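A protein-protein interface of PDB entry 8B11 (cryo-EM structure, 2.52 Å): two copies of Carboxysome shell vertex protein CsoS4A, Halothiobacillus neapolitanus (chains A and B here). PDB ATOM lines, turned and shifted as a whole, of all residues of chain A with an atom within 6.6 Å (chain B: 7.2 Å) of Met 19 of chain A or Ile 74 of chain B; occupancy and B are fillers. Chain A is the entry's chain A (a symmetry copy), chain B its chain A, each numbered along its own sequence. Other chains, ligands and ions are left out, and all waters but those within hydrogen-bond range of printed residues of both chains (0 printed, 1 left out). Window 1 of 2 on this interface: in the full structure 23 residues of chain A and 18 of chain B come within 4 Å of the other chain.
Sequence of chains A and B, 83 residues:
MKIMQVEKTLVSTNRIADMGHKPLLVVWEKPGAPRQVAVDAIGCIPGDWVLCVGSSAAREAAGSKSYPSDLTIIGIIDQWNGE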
ATOM      1  N   SER A  12     -33.910  -4.699 -15.532  1.00  0.00           N
ATOM      2  CA  SER A  12     -32.703  -4.044 -16.028  1.00  0.00           C
ATOM      3  C   SER A  12     -32.831  -3.975 -17.546  1.00  0.00           C
ATOM      4  O   SER A  12     -32.609  -4.969 -18.240  1.00  0.00           O
ATOM      5  CB  SER A  12     -31.448  -4.793 -15.597  1.00  0.00           C
ATOM      6  OG  SER A  12     -30.295  -4.253 -16.215  1.00  0.00           O
ATOM      7  N   ASN A  14     -31.083  -2.401 -19.907  1.00  0.00           N
ATOM      8  CA  ASN A  14     -29.874  -2.466 -20.718  1.00  0.00           C
ATOM      9  C   ASN A  14     -29.003  -3.678 -20.398  1.00  0.00           C
ATOM     10  O   ASN A  14     -27.813  -3.680 -20.727  1.00  0.00           O
ATOM     11  CB  ASN A  14     -29.060  -1.178 -20.569  1.00  0.00           C
ATOM     12  CG  ASN A  14     -28.386  -1.058 -19.220  1.00  0.00           C
ATOM     13  OD1 ASN A  14     -28.805  -1.673 -18.241  1.00  0.00           O
ATOM     14  ND2 ASN A  14     -27.333  -0.257 -19.162  1.00  0.00           N
ATOM     15  N   ARG A  15     -29.570  -4.709 -19.784  1.00  0.00           N
ATOM     16  CA  ARG A  15     -28.814  -5.907 -19.460  1.00  0.00           C
ATOM     17  C   ARG A  15     -28.332  -6.599 -20.733  1.00  0.00           C
ATOM     18  O   ARG A  15     -28.844  -6.369 -21.831  1.00  0.00           O
ATOM     19  CB  ARG A  15     -29.667  -6.860 -18.630  1.00  0.00           C
ATOM     20  CG  ARG A  15     -30.768  -7.525 -19.422  1.00  0.00           C
ATOM     21  CD  ARG A  15     -31.850  -8.066 -18.524  1.00  0.00           C
ATOM     22  NE  ARG A  15     -32.576  -9.163 -19.147  1.00  0.00           N
ATOM     23  CZ  ARG A  15     -33.453  -9.931 -18.513  1.00  0.00           C
ATOM     24  NH1 ARG A  15     -33.758  -9.726 -17.243  1.00  0.00           N
ATOM     25  NH2 ARG A  15     -34.037 -10.925 -19.170  1.00  0.00           N
ATOM     26  N   ILE A  16     -27.321  -7.455 -20.575  1.00  0.00           N
ATOM     27  CA  ILE A  16     -26.695  -8.070 -21.735  1.00  0.00           C
ATOM     28  C   ILE A  16     -27.708  -8.927 -22.489  1.00  0.00           C
ATOM     29  O   ILE A  16     -28.647  -9.484 -21.907  1.00  0.00           O
ATOM     30  CB  ILE A  16     -25.466  -8.904 -21.334  1.00  0.00           C
ATOM     31  CG1 ILE A  16     -25.830  -9.936 -20.270  1.00  0.00           C
ATOM     32  CG2 ILE A  16     -24.352  -8.000 -20.833  1.00  0.00           C
ATOM     33  CD1 ILE A  16     -24.665 -10.788 -19.826  1.00  0.00           C
ATOM     34  N   ALA A  17     -27.514  -9.025 -23.805  1.00  0.00           N
ATOM     35  CA  ALA A  17     -28.440  -9.771 -24.647  1.00  0.00           C
ATOM     36  C   ALA A  17     -28.467 -11.252 -24.312  1.00  0.00           C
ATOM     37  O   ALA A  17     -29.475 -11.916 -24.571  1.00  0.00           O
ATOM     38  CB  ALA A  17     -28.076  -9.584 -26.117  1.00  0.00           C
ATOM     39  N   ASP A  18     -27.385 -11.788 -23.746  1.00  0.00           N
ATOM     40  CA  ASP A  18     -27.325 -13.205 -23.417  1.00  0.00           C
ATOM     41  C   ASP A  18     -28.239 -13.581 -22.262  1.00  0.00           C
ATOM     42  O   ASP A  18     -28.437 -14.776 -22.016  1.00  0.00           O
ATOM     43  CB  ASP A  18     -25.885 -13.603 -23.100  1.00  0.00           C
ATOM     44  CG  ASP A  18     -25.004 -13.634 -24.338  1.00  0.00           C
ATOM     45  OD1 ASP A  18     -25.555 -13.591 -25.459  1.00  0.00           O
ATOM     46  OD2 ASP A  18     -23.765 -13.704 -24.191  1.00  0.00           O
ATOM     47  N   MET A  19     -28.798 -12.605 -21.550  1.00  0.00           N
ATOM     48  CA  MET A  19     -29.751 -12.885 -20.490  1.00  0.00           C
ATOM     49  C   MET A  19     -31.113 -13.308 -21.024  1.00  0.00           C
ATOM     50  O   MET A  19     -31.951 -13.767 -20.242  1.00  0.00           O
ATOM     51  CB  MET A  19     -29.904 -11.659 -19.589  1.00  0.00           C
ATOM     52  CG  MET A  19     -28.920 -11.630 -18.433  1.00  0.00           C
ATOM     53  SD  MET A  19     -29.519 -10.755 -16.985  1.00  0.00           S
ATOM     54  CE  MET A  19     -29.761 -12.122 -15.861  1.00  0.00           C
ATOM     55  N   GLY A  20     -31.350 -13.167 -22.328  1.00  0.00           N
ATOM     56  CA  GLY A  20     -32.597 -13.615 -22.920  1.00  0.00           C
ATOM     57  C   GLY A  20     -33.781 -12.802 -22.439  1.00  0.00           C
ATOM     58  O   GLY A  20     -33.672 -11.610 -22.138  1.00  0.00           O
ATOM     59  N   HIS A  21     -34.936 -13.458 -22.367  1.00  0.00           N
ATOM     60  CA  HIS A  21     -36.169 -12.838 -21.901  1.00  0.00           C
ATOM     61  C   HIS A  21     -36.531 -13.272 -20.487  1.00  0.00           C
ATOM     62  O   HIS A  21     -37.663 -13.056 -20.048  1.00  0.00           O
ATOM     63  CB  HIS A  21     -37.319 -13.158 -22.855  1.00  0.00           C
ATOM     64  CG  HIS A  21     -37.106 -12.671 -24.255  1.00  0.00           C
ATOM     65  ND1 HIS A  21     -37.885 -13.085 -25.312  1.00  0.00           N
ATOM     66  CD2 HIS A  21     -36.198 -11.811 -24.773  1.00  0.00           C
ATOM     67  CE1 HIS A  21     -37.470 -12.495 -26.420  1.00  0.00           C
ATOM     68  NE2 HIS A  21     -36.449 -11.717 -26.119  1.00  0.00           N
ATOM     69  N   LYS A  22     -35.597 -13.879 -19.768  1.00  0.00           N
ATOM     70  CA  LYS A  22     -35.926 -14.516 -18.503  1.00  0.00           C
ATOM     71  C   LYS A  22     -36.156 -13.468 -17.418  1.00  0.00           C
ATOM     72  O   LYS A  22     -35.412 -12.489 -17.330  1.00  0.00           O
ATOM     73  CB  LYS A  22     -34.811 -15.468 -18.085  1.00  0.00           C
ATOM     74  CG  LYS A  22     -34.805 -16.761 -18.869  1.00  0.00           C
ATOM     75  CD  LYS A  22     -34.503 -17.955 -17.989  1.00  0.00           C
ATOM     76  CE  LYS A  22     -35.778 -18.653 -17.551  1.00  0.00           C
ATOM     77  NZ  LYS A  22     -36.678 -18.902 -18.709  1.00  0.00           N
ATOM     78  N   PRO A  23     -37.174 -13.643 -16.583  1.00  0.00           N
ATOM     79  CA  PRO A  23     -37.441 -12.664 -15.525  1.00  0.00           C
ATOM     80  C   PRO A  23     -36.444 -12.776 -14.384  1.00  0.00           C
ATOM     81  O   PRO A  23     -35.836 -13.821 -14.138  1.00  0.00           O
ATOM     82  CB  PRO A  23     -38.853 -13.023 -15.053  1.00  0.00           C
ATOM     83  CG  PRO A  23     -39.378 -14.009 -16.055  1.00  0.00           C
ATOM     84  CD  PRO A  23     -38.195 -14.695 -16.623  1.00  0.00           C
ATOM     85  N   LEU A  24     -36.303 -11.669 -13.661  1.00  0.00           N
ATOM     86  CA  LEU A  24     -35.390 -11.562 -12.533  1.00  0.00           C
ATOM     87  C   LEU A  24     -36.168 -11.176 -11.286  1.00  0.00           C
ATOM     88  O   LEU A  24     -36.980 -10.248 -11.318  1.00  0.00           O
ATOM     89  CB  LEU A  24     -34.293 -10.532 -12.802  1.00  0.00           C
ATOM     90  CG  LEU A  24     -33.383 -10.823 -13.991  1.00  0.00           C
ATOM     91  CD1 LEU A  24     -32.335  -9.736 -14.132  1.00  0.00           C
ATOM     92  CD2 LEU A  24     -32.738 -12.185 -13.836  1.00  0.00           C
ATOM     93  N   VAL A  37     -30.415 -11.415  -6.491  1.00  0.00           N
ATOM     94  CA  VAL A  37     -31.249 -11.483  -7.681  1.00  0.00           C
ATOM     95  C   VAL A  37     -31.136 -12.882  -8.265  1.00  0.00           C
ATOM     96  O   VAL A  37     -30.029 -13.377  -8.498  1.00  0.00           O
ATOM     97  CB  VAL A  37     -30.856 -10.413  -8.713  1.00  0.00           C
ATOM     98  CG1 VAL A  37     -31.742 -10.513  -9.941  1.00  0.00           C
ATOM     99  CG2 VAL A  37     -30.959  -9.039  -8.090  1.00  0.00           C
ATOM    100  N   VAL A  39     -32.644 -15.685 -11.297  1.00  0.00           N
ATOM    101  CA  VAL A  39     -33.370 -15.923 -12.538  1.00  0.00           C
ATOM    102  C   VAL A  39     -34.589 -16.775 -12.210  1.00  0.00           C
ATOM    103  O   VAL A  39     -34.465 -17.838 -11.594  1.00  0.00           O
ATOM    104  CB  VAL A  39     -32.477 -16.606 -13.582  1.00  0.00           C
ATOM    105  CG1 VAL A  39     -33.307 -17.122 -14.741  1.00  0.00           C
ATOM    106  CG2 VAL A  39     -31.412 -15.642 -14.077  1.00  0.00           C
ATOM    107  N   TYR A  67     -25.678 -19.706 -20.095  1.00  0.00           N
ATOM    108  CA  TYR A  67     -26.515 -18.635 -19.565  1.00  0.00           C
ATOM    109  C   TYR A  67     -25.792 -17.886 -18.450  1.00  0.00           C
ATOM    110  O   TYR A  67     -25.186 -18.515 -17.577  1.00  0.00           O
ATOM    111  CB  TYR A  67     -27.843 -19.184 -19.054  1.00  0.00           C
ATOM    112  CG  TYR A  67     -28.863 -18.096 -18.841  1.00  0.00           C
ATOM    113  CD1 TYR A  67     -28.924 -17.400 -17.642  1.00  0.00           C
ATOM    114  CD2 TYR A  67     -29.738 -17.733 -19.853  1.00  0.00           C
ATOM    115  CE1 TYR A  67     -29.839 -16.397 -17.448  1.00  0.00           C
ATOM    116  CE2 TYR A  67     -30.655 -16.728 -19.668  1.00  0.00           C
ATOM    117  CZ  TYR A  67     -30.701 -16.064 -18.466  1.00  0.00           C
ATOM    118  OH  TYR A  67     -31.616 -15.058 -18.277  1.00  0.00           O
ATOM    119  N   PRO A  68     -25.838 -16.550 -18.440  1.00  0.00           N
ATOM    120  CA  PRO A  68     -25.190 -15.744 -17.384  1.00  0.00           C
ATOM    121  C   PRO A  68     -26.013 -15.634 -16.102  1.00  0.00           C
ATOM    122  O   PRO A  68     -26.578 -14.601 -15.754  1.00  0.00           O
ATOM    123  CB  PRO A  68     -25.024 -14.384 -18.064  1.00  0.00           C
ATOM    124  CG  PRO A  68     -26.190 -14.304 -18.980  1.00  0.00           C
ATOM    125  CD  PRO A  68     -26.448 -15.702 -19.477  1.00  0.00           C
ATOM    126  N   SER A  69     -26.086 -16.739 -15.369  1.00  0.00           N
ATOM    127  CA  SER A  69     -26.784 -16.776 -14.093  1.00  0.00           C
ATOM    128  C   SER A  69     -25.922 -17.487 -13.066  1.00  0.00           C
ATOM    129  O   SER A  69     -25.332 -18.528 -13.359  1.00  0.00           O
ATOM    130  CB  SER A  69     -28.141 -17.482 -14.212  1.00  0.00           C
ATOM    131  OG  SER A  69     -28.792 -17.551 -12.956  1.00  0.00           O
ATOM    132  N   MET B   1     -27.119 -13.772  -8.562  1.00  0.00           N
ATOM    133  CA  MET B   1     -26.539 -12.456  -8.786  1.00  0.00           C
ATOM    134  C   MET B   1     -26.736 -11.528  -7.594  1.00  0.00           C
ATOM    135  O   MET B   1     -27.611 -11.736  -6.761  1.00  0.00           O
ATOM    136  CB  MET B   1     -27.119 -11.828 -10.052  1.00  0.00           C
ATOM    137  CG  MET B   1     -27.098 -12.746 -11.269  1.00  0.00           C
ATOM    138  SD  MET B   1     -28.074 -14.252 -11.104  1.00  0.00           S
ATOM    139  CE  MET B   1     -29.632 -13.722 -11.797  1.00  0.00           C
ATOM    140  N   VAL B  39     -15.746  -6.847 -13.817  1.00  0.00           N
ATOM    141  CA  VAL B  39     -15.551  -6.540 -15.228  1.00  0.00           C
ATOM    142  C   VAL B  39     -16.788  -5.801 -15.720  1.00  0.00           C
ATOM    143  O   VAL B  39     -17.914  -6.280 -15.553  1.00  0.00           O
ATOM    144  CB  VAL B  39     -15.299  -7.814 -16.044  1.00  0.00           C
ATOM    145  CG1 VAL B  39     -15.403  -7.527 -17.529  1.00  0.00           C
ATOM    146  CG2 VAL B  39     -13.938  -8.398 -15.708  1.00  0.00           C
ATOM    147  N   ASP B  40     -16.585  -4.626 -16.308  1.00  0.00           N
ATOM    148  CA  ASP B  40     -17.689  -3.776 -16.744  1.00  0.00           C
ATOM    149  C   ASP B  40     -18.064  -4.156 -18.168  1.00  0.00           C
ATOM    150  O   ASP B  40     -17.520  -3.630 -19.139  1.00  0.00           O
ATOM    151  CB  ASP B  40     -17.300  -2.308 -16.641  1.00  0.00           C
ATOM    152  CG  ASP B  40     -18.470  -1.379 -16.837  1.00  0.00           C
ATOM    153  OD1 ASP B  40     -19.627  -1.847 -16.784  1.00  0.00           O
ATOM    154  OD2 ASP B  40     -18.231  -0.174 -17.046  1.00  0.00           O
ATOM    155  N   ALA B  41     -19.013  -5.075 -18.299  1.00  0.00           N
ATOM    156  CA  ALA B  41     -19.528  -5.466 -19.602  1.00  0.00           C
ATOM    157  C   ALA B  41     -20.654  -4.563 -20.082  1.00  0.00           C
ATOM    158  O   ALA B  41     -21.178  -4.778 -21.179  1.00  0.00           O
ATOM    159  CB  ALA B  41     -20.011  -6.918 -19.566  1.00  0.00           C
ATOM    160  N   ILE B  42     -21.029  -3.553 -19.297  1.00  0.00           N
ATOM    161  CA  ILE B  42     -22.169  -2.702 -19.592  1.00  0.00           C
ATOM    162  C   ILE B  42     -21.751  -1.270 -19.901  1.00  0.00           C
ATOM    163  O   ILE B  42     -22.304  -0.643 -20.811  1.00  0.00           O
ATOM    164  CB  ILE B  42     -23.193  -2.729 -18.435  1.00  0.00           C
ATOM    165  CG1 ILE B  42     -23.867  -4.096 -18.363  1.00  0.00           C
ATOM    166  CG2 ILE B  42     -24.238  -1.646 -18.607  1.00  0.00           C
ATOM    167  CD1 ILE B  42     -24.630  -4.459 -19.614  1.00  0.00           C
ATOM    168  N   VAL B  50     -26.047  -1.772 -10.050  1.00  0.00           N
ATOM    169  CA  VAL B  50     -25.776  -2.706 -11.128  1.00  0.00           C
ATOM    170  C   VAL B  50     -26.027  -4.124 -10.646  1.00  0.00           C
ATOM    171  O   VAL B  50     -26.069  -4.407  -9.447  1.00  0.00           O
ATOM    172  CB  VAL B  50     -24.333  -2.567 -11.664  1.00  0.00           C
ATOM    173  CG1 VAL B  50     -24.128  -1.203 -12.288  1.00  0.00           C
ATOM    174  CG2 VAL B  50     -23.326  -2.810 -10.558  1.00  0.00           C
ATOM    175  N   LEU B  51     -26.194  -5.015 -11.613  1.00  0.00           N
ATOM    176  CA  LEU B  51     -26.319  -6.443 -11.380  1.00  0.00           C
ATOM    177  C   LEU B  51     -24.975  -7.097 -11.647  1.00  0.00           C
ATOM    178  O   LEU B  51     -24.377  -6.877 -12.702  1.00  0.00           O
ATOM    179  CB  LEU B  51     -27.384  -7.053 -12.289  1.00  0.00           C
ATOM    180  CG  LEU B  51     -28.760  -7.262 -11.676  1.00  0.00           C
ATOM    181  CD1 LEU B  51     -29.789  -7.456 -12.773  1.00  0.00           C
ATOM    182  CD2 LEU B  51     -28.725  -8.445 -10.734  1.00  0.00           C
ATOM    183  N   CYS B  52     -24.498  -7.885 -10.692  1.00  0.00           N
ATOM    184  CA  CYS B  52     -23.208  -8.543 -10.809  1.00  0.00           C
ATOM    185  C   CYS B  52     -23.401 -10.044 -10.682  1.00  0.00           C
ATOM    186  O   CYS B  52     -24.055 -10.513  -9.748  1.00  0.00           O
ATOM    187  CB  CYS B  52     -22.237  -8.029  -9.748  1.00  0.00           C
ATOM    188  SG  CYS B  52     -21.782  -6.297  -9.962  1.00  0.00           S
ATOM    189  N   VAL B  53     -22.831 -10.792 -11.616  1.00  0.00           N
ATOM    190  CA  VAL B  53     -22.872 -12.244 -11.591  1.00  0.00           C
ATOM    191  C   VAL B  53     -21.472 -12.752 -11.280  1.00  0.00           C
ATOM    192  O   VAL B  53     -20.478 -12.238 -11.806  1.00  0.00           O
ATOM    193  CB  VAL B  53     -23.412 -12.820 -12.918  1.00  0.00           C
ATOM    194  CG1 VAL B  53     -22.513 -12.461 -14.086  1.00  0.00           C
ATOM    195  CG2 VAL B  53     -23.595 -14.319 -12.816  1.00  0.00           C
ATOM    196  N   ALA B  57     -20.319 -17.896 -14.672  1.00  0.00           N
ATOM    197  CA  ALA B  57     -21.129 -17.134 -15.613  1.00  0.00           C
ATOM    198  C   ALA B  57     -20.506 -15.781 -15.921  1.00  0.00           C
ATOM    199  O   ALA B  57     -20.736 -15.225 -17.000  1.00  0.00           O
ATOM    200  CB  ALA B  57     -22.544 -16.954 -15.068  1.00  0.00           C
ATOM    201  N   ALA B  58     -19.718 -15.240 -14.988  1.00  0.00           N
ATOM    202  CA  ALA B  58     -19.052 -13.965 -15.220  1.00  0.00           C
ATOM    203  C   ALA B  58     -18.039 -14.052 -16.351  1.00  0.00           C
ATOM    204  O   ALA B  58     -17.764 -13.047 -17.013  1.00  0.00           O
ATOM    205  CB  ALA B  58     -18.368 -13.488 -13.939  1.00  0.00           C
ATOM    206  N   GLU B  60     -18.208 -15.875 -19.291  1.00  0.00           N
ATOM    207  CA  GLU B  60     -18.907 -15.692 -20.555  1.00  0.00           C
ATOM    208  C   GLU B  60     -19.599 -14.340 -20.616  1.00  0.00           C
ATOM    209  O   GLU B  60     -19.717 -13.755 -21.698  1.00  0.00           O
ATOM    210  CB  GLU B  60     -19.920 -16.814 -20.761  1.00  0.00           C
ATOM    211  CG  GLU B  60     -19.428 -17.937 -21.643  1.00  0.00           C
ATOM    212  CD  GLU B  60     -19.777 -17.727 -23.099  1.00  0.00           C
ATOM    213  OE1 GLU B  60     -20.792 -18.293 -23.551  1.00  0.00           O
ATOM    214  OE2 GLU B  60     -19.038 -16.999 -23.795  1.00  0.00           O
ATOM    215  N   ALA B  61     -20.060 -13.832 -19.470  1.00  0.00           N
ATOM    216  CA  ALA B  61     -20.635 -12.493 -19.435  1.00  0.00           C
ATOM    217  C   ALA B  61     -19.617 -11.442 -19.853  1.00  0.00           C
ATOM    218  O   ALA B  61     -19.993 -10.396 -20.391  1.00  0.00           O
ATOM    219  CB  ALA B  61     -21.171 -12.193 -18.036  1.00  0.00           C
ATOM    220  N   ALA B  62     -18.331 -11.705 -19.624  1.00  0.00           N
ATOM    221  CA  ALA B  62     -17.267 -10.798 -20.031  1.00  0.00           C
ATOM    222  C   ALA B  62     -16.774 -11.056 -21.448  1.00  0.00           C
ATOM    223  O   ALA B  62     -15.900 -10.325 -21.920  1.00  0.00           O
ATOM    224  CB  ALA B  62     -16.094 -10.887 -19.054  1.00  0.00           C
ATOM    225  N   THR B  72     -18.743  -9.994 -12.960  1.00  0.00           N
ATOM    226  CA  THR B  72     -18.998  -9.190 -14.146  1.00  0.00           C
ATOM    227  C   THR B  72     -20.314  -8.449 -13.974  1.00  0.00           C
ATOM    228  O   THR B  72     -21.303  -9.033 -13.522  1.00  0.00           O
ATOM    229  CB  THR B  72     -19.037 -10.065 -15.409  1.00  0.00           C
ATOM    230  OG1 THR B  72     -17.755 -10.657 -15.623  1.00  0.00           O
ATOM    231  CG2 THR B  72     -19.417  -9.252 -16.629  1.00  0.00           C
ATOM    232  N   ILE B  73     -20.321  -7.166 -14.317  1.00  0.00           N
ATOM    233  CA  ILE B  73     -21.555  -6.392 -14.367  1.00  0.00           C
ATOM    234  C   ILE B  73     -22.301  -6.749 -15.645  1.00  0.00           C
ATOM    235  O   ILE B  73     -21.741  -6.679 -16.745  1.00  0.00           O
ATOM    236  CB  ILE B  73     -21.259  -4.887 -14.298  1.00  0.00           C
ATOM    237  CG1 ILE B  73     -20.614  -4.531 -12.960  1.00  0.00           C
ATOM    238  CG2 ILE B  73     -22.529  -4.085 -14.510  1.00  0.00           C
ATOM    239  CD1 ILE B  73     -19.927  -3.209 -12.960  1.00  0.00           C
ATOM    240  N   ILE B  74     -23.564  -7.145 -15.509  1.00  0.00           N
ATOM    241  CA  ILE B  74     -24.360  -7.582 -16.647  1.00  0.00           C
ATOM    242  C   ILE B  74     -25.589  -6.719 -16.878  1.00  0.00           C
ATOM    243  O   ILE B  74     -26.363  -7.005 -17.791  1.00  0.00           O
ATOM    244  CB  ILE B  74     -24.769  -9.065 -16.519  1.00  0.00           C
ATOM    245  CG1 ILE B  74     -25.525  -9.315 -15.214  1.00  0.00           C
ATOM    246  CG2 ILE B  74     -23.557  -9.957 -16.616  1.00  0.00           C
ATOM    247  CD1 ILE B  74     -26.244 -10.636 -15.192  1.00  0.00           C
ATOM    248  N   GLY B  75     -25.794  -5.679 -16.086  1.00  0.00           N
ATOM    249  CA  GLY B  75     -26.913  -4.792 -16.320  1.00  0.00           C
ATOM    250  C   GLY B  75     -26.948  -3.681 -15.297  1.00  0.00           C
ATOM    251  O   GLY B  75     -26.369  -3.784 -14.214  1.00  0.00           O
ATOM    252  N   ILE B  76     -27.648  -2.614 -15.664  1.00  0.00           N
ATOM    253  CA  ILE B  76     -27.906  -1.483 -14.784  1.00  0.00           C
ATOM    254  C   ILE B  76     -29.366  -1.545 -14.364  1.00  0.00           C
ATOM    255  O   ILE B  76     -30.253  -1.678 -15.213  1.00  0.00           O
ATOM    256  CB  ILE B  76     -27.596  -0.144 -15.472  1.00  0.00           C
ATOM    257  CG1 ILE B  76     -26.121  -0.068 -15.852  1.00  0.00           C
ATOM    258  CG2 ILE B  76     -27.975   1.019 -14.567  1.00  0.00           C
ATOM    259  CD1 ILE B  76     -25.742   1.224 -16.524  1.00  0.00           C
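Met 19 of chain A touches just one residue of chain B: Ile 74. Printed residues of chain A within 4 Å of Ile 74 of chain B: Arg 15, Ile 16 and Met 19. Of the printed residues of chain B, Val 37 of chain A touches Met 1 (2.8 Å) and Leu 51 (3.5 Å). Of the printed residues of chain B, Ser 69 of chain A touches Met 1 (3.9 Å), Val 53 (3.9 Å) and Ala 57 (3.6 Å). Of the printed residues of chain A, Leu 51 of chain B touches Leu 24 and Val 37. Pro 23 of chain A touches none of the printed residues of chain B. The nearest residue of chain B that does not touch Met 19 of chain A is Met 1 of chain B (4.4 Å). The nearest printed residue of chain A that does not touch Ile 74 of chain B is Pro 68 of chain A (4.02 Å).
O of Ile 74 of chain B sits at hydrogen-bond distance from N of Ile 16 of chain A (3.0 Å). O of Met 1 of chain B is in hydrogen-bond range of N of Val 37 of chain A (2.8 Å). O of Ile 76 of chain B sits at hydrogen-bond distance from OG of Ser 12 of chain A, at 2.8 Å. The side-chain amide oxygen (OD1) of Asn 14 of chain A sits at hydrogen-bond distance from the backbone NH (N) of Ile 76 of chain B (3.0 Å).
Among the printed residues, merely in contact across the chains: Ser 12 of chain A with Gly 75 of chain B (3.4 Å), Asn 14 of chain A with Ile 42 of chain B (3.4 Å), Arg 15 of chain A with Ile 74 of chain B (3.2 Å), Arg 15 of chain A with Gly 75 of chain B (3.8 Å), Ile 16 of chain A with Ile 42 of chain B (3.8 Å), Met 19 of chain A with Ile 74 of chain B (3.7 Å), Leu 24 of chain A with Leu 51 of chain B (3.7 Å), Val 37 of chain A with Leu 51 of chain B (3.5 Å), Val 39 of chain A with Met 1 of chain B (3.5 Å), Tyr 67 of chain A with Ala 57 of chain B (3.96 Å), Pro 68 of chain A with Ala 57 of chain B (3.7 Å), Ser 69 of chain A with Met 1 of chain B (3.9 Å), Ser 69 of chain A with Val 53 of chain B (3.9 Å) and Ser 69 of chain A with Ala 57 of chain B (3.6 Å).
NH2 of Arg 15 of chain A lies within hydrogen-bond range of O of Gly 20 of chain A. O of Lys 22 of chain A sits at hydrogen-bond distance from NH2 of Arg 15 of chain A, 2.8 Å away. O of Thr 72 of chain B is in hydrogen-bond range of N of Val 53 of chain B, at 3.0 Å. The backbone NH (N) of Leu 51 of chain B lies within hydrogen-bond range of the backbone carbonyl oxygen (O) of Gly 75 of chain B. The backbone carbonyl oxygen (O) of Leu 51 of chain B sits at hydrogen-bond distance from the backbone NH (N) of Ile 74 of chain B, 2.9 Å away. The backbone NH of Ile 42 of chain B lies close to the side-chain carboxylate of Asp 40 of chain B (3.3 Å).
Of the 17 printed residues of chain A, 11 touch a printed residue of chain B. Hydrophobic or aromatic side chains of chain A that line the printed part of chain B: Ile 16, Met 19, Leu 24, Val 37 and Val 39. Hydrophobic or aromatic side chains of chain B within 4 Å of the printed part of chain A: Met 1, Ile 42, Leu 51, Val 53, Ala 57, Ile 74 and Ile 76. Among the printed residues, no Asp or Glu carboxylate lies within 4 Å of a Lys or Arg side-chain nitrogen of the other chain.
1 position is printed for both chains.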
